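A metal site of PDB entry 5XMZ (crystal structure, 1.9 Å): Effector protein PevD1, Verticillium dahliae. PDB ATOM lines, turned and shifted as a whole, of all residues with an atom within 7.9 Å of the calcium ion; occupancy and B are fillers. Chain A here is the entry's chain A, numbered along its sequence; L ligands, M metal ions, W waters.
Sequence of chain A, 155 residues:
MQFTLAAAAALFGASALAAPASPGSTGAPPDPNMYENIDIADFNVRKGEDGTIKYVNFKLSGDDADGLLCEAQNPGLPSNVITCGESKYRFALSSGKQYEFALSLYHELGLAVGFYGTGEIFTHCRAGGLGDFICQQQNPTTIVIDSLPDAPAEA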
ATOM      1  N   ASP A  31       0.784  29.868  -9.319  1.00  0.00           N
ATOM      2  CA  ASP A  31       0.246  30.480  -8.109  1.00  0.00           C
ATOM      3  C   ASP A  31       0.753  31.909  -7.872  1.00  0.00           C
ATOM      4  O   ASP A  31      -0.057  32.807  -7.680  1.00  0.00           O
ATOM      5  CB  ASP A  31       0.508  29.591  -6.871  1.00  0.00           C
ATOM      6  CG  ASP A  31      -0.401  29.936  -5.701  1.00  0.00           C
ATOM      7  OD1 ASP A  31      -0.927  31.063  -5.640  1.00  0.00           O
ATOM      8  OD2 ASP A  31      -0.588  29.068  -4.827  1.00  0.00           O
ATOM      9  N   LEU A 105     -13.704  26.658  -4.670  1.00  0.00           N
ATOM     10  CA  LEU A 105     -14.216  27.624  -5.639  1.00  0.00           C
ATOM     11  C   LEU A 105     -13.593  27.333  -6.981  1.00  0.00           C
ATOM     12  O   LEU A 105     -12.436  26.950  -7.042  1.00  0.00           O
ATOM     13  CB  LEU A 105     -13.817  29.033  -5.218  1.00  0.00           C
ATOM     14  CG  LEU A 105     -14.349  29.510  -3.869  1.00  0.00           C
ATOM     15  CD1 LEU A 105     -13.529  30.702  -3.407  1.00  0.00           C
ATOM     16  CD2 LEU A 105     -15.820  29.865  -3.995  1.00  0.00           C
ATOM     17  N   GLY A 114      -9.053  25.162 -15.765  1.00  0.00           N
ATOM     18  CA  GLY A 114      -9.845  26.156 -15.048  1.00  0.00           C
ATOM     19  C   GLY A 114      -9.155  26.575 -13.771  1.00  0.00           C
ATOM     20  O   GLY A 114      -8.168  25.970 -13.374  1.00  0.00           O
ATOM     21  N   PHE A 115      -9.677  27.623 -13.131  1.00  0.00           N
ATOM     22  CA  PHE A 115      -9.142  28.076 -11.856  1.00  0.00           C
ATOM     23  C   PHE A 115      -9.859  27.342 -10.711  1.00  0.00           C
ATOM     24  O   PHE A 115     -11.067  27.050 -10.779  1.00  0.00           O
ATOM     25  CB  PHE A 115      -9.314  29.594 -11.684  1.00  0.00           C
ATOM     26  CG  PHE A 115      -8.150  30.417 -12.218  1.00  0.00           C
ATOM     27  CD1 PHE A 115      -7.068  29.816 -12.852  1.00  0.00           C
ATOM     28  CD2 PHE A 115      -8.139  31.793 -12.052  1.00  0.00           C
ATOM     29  CE1 PHE A 115      -6.006  30.581 -13.330  1.00  0.00           C
ATOM     30  CE2 PHE A 115      -7.079  32.574 -12.517  1.00  0.00           C
ATOM     31  CZ  PHE A 115      -5.999  31.951 -13.157  1.00  0.00           C
ATOM     32  N   TYR A 116      -9.108  27.029  -9.671  1.00  0.00           N
ATOM     33  CA  TYR A 116      -9.623  26.302  -8.522  1.00  0.00           C
ATOM     34  C   TYR A 116      -8.861  26.713  -7.274  1.00  0.00           C
ATOM     35  O   TYR A 116      -7.674  27.051  -7.345  1.00  0.00           O
ATOM     36  CB  TYR A 116      -9.472  24.792  -8.754  1.00  0.00           C
ATOM     37  CG  TYR A 116      -9.529  23.991  -7.479  1.00  0.00           C
ATOM     38  CD1 TYR A 116     -10.734  23.692  -6.865  1.00  0.00           C
ATOM     39  CD2 TYR A 116      -8.351  23.523  -6.888  1.00  0.00           C
ATOM     40  CE1 TYR A 116     -10.778  22.961  -5.692  1.00  0.00           C
ATOM     41  CE2 TYR A 116      -8.380  22.789  -5.725  1.00  0.00           C
ATOM     42  CZ  TYR A 116      -9.596  22.519  -5.133  1.00  0.00           C
ATOM     43  OH  TYR A 116      -9.622  21.791  -3.977  1.00  0.00           O
ATOM     44  N   GLY A 117      -9.527  26.718  -6.127  1.00  0.00           N
ATOM     45  CA  GLY A 117      -8.843  26.921  -4.871  1.00  0.00           C
ATOM     46  C   GLY A 117      -9.791  26.726  -3.709  1.00  0.00           C
ATOM     47  O   GLY A 117     -11.003  26.715  -3.887  1.00  0.00           O
ATOM     48  N   THR A 118      -9.228  26.557  -2.521  1.00  0.00           N
ATOM     49  CA  THR A 118     -10.010  26.217  -1.348  1.00  0.00           C
ATOM     50  C   THR A 118      -9.565  27.083  -0.182  1.00  0.00           C
ATOM     51  O   THR A 118      -8.395  27.428  -0.073  1.00  0.00           O
ATOM     52  CB  THR A 118      -9.803  24.725  -0.922  1.00  0.00           C
ATOM     53  OG1 THR A 118     -10.139  23.852  -2.000  1.00  0.00           O
ATOM     54  CG2 THR A 118     -10.673  24.372   0.255  1.00  0.00           C
ATOM     55  N   VAL A 144      -7.632  32.539  -2.660  1.00  0.00           N
ATOM     56  CA  VAL A 144      -6.926  32.625  -3.946  1.00  0.00           C
ATOM     57  C   VAL A 144      -7.174  31.359  -4.747  1.00  0.00           C
ATOM     58  O   VAL A 144      -6.972  30.239  -4.255  1.00  0.00           O
ATOM     59  CB  VAL A 144      -5.403  32.777  -3.738  1.00  0.00           C
ATOM     60  CG1 VAL A 144      -4.680  32.735  -5.071  1.00  0.00           C
ATOM     61  CG2 VAL A 144      -5.101  34.058  -2.997  1.00  0.00           C
ATOM     62  N   ILE A 145      -7.621  31.525  -5.994  1.00  0.00           N
ATOM     63  CA  ILE A 145      -7.735  30.401  -6.903  1.00  0.00           C
ATOM     64  C   ILE A 145      -6.737  30.538  -8.050  1.00  0.00           C
ATOM     65  O   ILE A 145      -6.312  31.641  -8.414  1.00  0.00           O
ATOM     66  CB  ILE A 145      -9.184  30.223  -7.436  1.00  0.00           C
ATOM     67  CG1 ILE A 145      -9.595  31.384  -8.328  1.00  0.00           C
ATOM     68  CG2 ILE A 145     -10.160  30.106  -6.247  1.00  0.00           C
ATOM     69  CD1 ILE A 145     -11.043  31.272  -8.831  1.00  0.00           C
ATOM     70  N   ASP A 146      -6.352  29.397  -8.611  1.00  0.00           N
ATOM     71  CA  ASP A 146      -5.398  29.380  -9.701  1.00  0.00           C
ATOM     72  C   ASP A 146      -5.525  28.073 -10.465  1.00  0.00           C
ATOM     73  O   ASP A 146      -6.420  27.265 -10.184  1.00  0.00           O
ATOM     74  CB  ASP A 146      -3.966  29.610  -9.188  1.00  0.00           C
ATOM     75  CG  ASP A 146      -3.525  28.552  -8.179  1.00  0.00           C
ATOM     76  OD1 ASP A 146      -3.927  27.393  -8.287  1.00  0.00           O
ATOM     77  OD2 ASP A 146      -2.736  28.887  -7.264  1.00  0.00           O
ATOM     78  N   SER A 147      -4.639  27.839 -11.424  1.00  0.00           N
ATOM     79  CA  SER A 147      -4.771  26.644 -12.248  1.00  0.00           C
ATOM     80  C   SER A 147      -3.960  25.474 -11.720  1.00  0.00           C
ATOM     81  O   SER A 147      -3.703  24.518 -12.449  1.00  0.00           O
ATOM     82  CB  SER A 147      -4.347  26.930 -13.679  1.00  0.00           C
ATOM     83  OG  SER A 147      -2.958  27.198 -13.715  1.00  0.00           O
ATOM     84  N   LEU A 148      -3.516  25.554 -10.474  1.00  0.00           N
ATOM     85  CA  LEU A 148      -2.839  24.420  -9.880  1.00  0.00           C
ATOM     86  C   LEU A 148      -3.817  23.597  -9.047  1.00  0.00           C
ATOM     87  O   LEU A 148      -4.791  24.122  -8.511  1.00  0.00           O
ATOM     88  CB  LEU A 148      -1.675  24.872  -9.009  1.00  0.00           C
ATOM     89  CG  LEU A 148      -0.625  25.717  -9.732  1.00  0.00           C
ATOM     90  CD1 LEU A 148       0.403  26.202  -8.729  1.00  0.00           C
ATOM     91  CD2 LEU A 148       0.034  24.896 -10.826  1.00  0.00           C
ATOM     92  N   PRO A 149      -3.546  22.281  -8.944  1.00  0.00           N
ATOM     93  CA  PRO A 149      -4.377  21.419  -8.089  1.00  0.00           C
ATOM     94  C   PRO A 149      -4.020  21.621  -6.624  1.00  0.00           C
ATOM     95  O   PRO A 149      -3.225  22.513  -6.320  1.00  0.00           O
ATOM     96  CB  PRO A 149      -3.983  20.016  -8.548  1.00  0.00           C
ATOM     97  CG  PRO A 149      -2.555  20.164  -9.005  1.00  0.00           C
ATOM     98  CD  PRO A 149      -2.458  21.541  -9.597  1.00  0.00           C
ATOM     99  N   ASP A 150      -4.606  20.818  -5.743  1.00  0.00           N
ATOM    100  CA  ASP A 150      -4.370  20.939  -4.306  1.00  0.00           C
ATOM    101  C   ASP A 150      -2.911  20.658  -3.954  1.00  0.00           C
ATOM    102  O   ASP A 150      -2.284  19.774  -4.543  1.00  0.00           O
ATOM    103  CB  ASP A 150      -5.276  19.985  -3.524  1.00  0.00           C
ATOM    104  CG  ASP A 150      -6.716  20.455  -3.467  1.00  0.00           C
ATOM    105  OD1 ASP A 150      -6.943  21.632  -3.137  1.00  0.00           O
ATOM    106  OD2 ASP A 150      -7.608  19.638  -3.766  1.00  0.00           O
ATOM    107  N   ALA A 151      -2.390  21.417  -2.998  1.00  0.00           N
ATOM    108  CA  ALA A 151      -1.084  21.127  -2.417  1.00  0.00           C
ATOM    109  C   ALA A 151      -1.188  19.805  -1.655  1.00  0.00           C
ATOM    110  O   ALA A 151      -2.248  19.481  -1.133  1.00  0.00           O
ATOM    111  CB  ALA A 151      -0.657  22.247  -1.489  1.00  0.00           C
HETATM  112 CL1  LIG L   1      -4.935  24.789  -5.230  1.00  0.00          CL
HETATM  113 CA    CA M   1      -5.512  25.913  -7.382  1.00  0.00          CA
HETATM  114  O   HOH W   1      -2.696  26.612  -5.795  1.00  0.00           O
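The side-chain carboxylate of Asp 150 sits at hydrogen-bond distance from the side-chain hydroxyl of Tyr 116.
The side-chain hydroxyl (OH) of Tyr 116 lies within hydrogen-bond range of the side-chain hydroxyl (OG1) of Thr 118, at 2.9 Å.
Of the 15 residues printed, 3 come within 4 Å of the calcium ion.
Along chain A the residues within 4 Å of the calcium ion span positions 116 to 148.
The calcium ion is bound by the backbone carbonyl oxygen of Leu 148 (2.2 Å), the side-chain carboxylate of Asp 146 (2.3 Å), the backbone carbonyl oxygen of Tyr 116 (2.4 Å) and a chlorine (CL1) of the ligand (2.5 Å).
The calcium ion has four donor atoms within binding distance.
Water W1 lies within hydrogen-bond range of the side-chain carboxylate of Asp 146 and the side-chain carboxylate of Asp 31.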
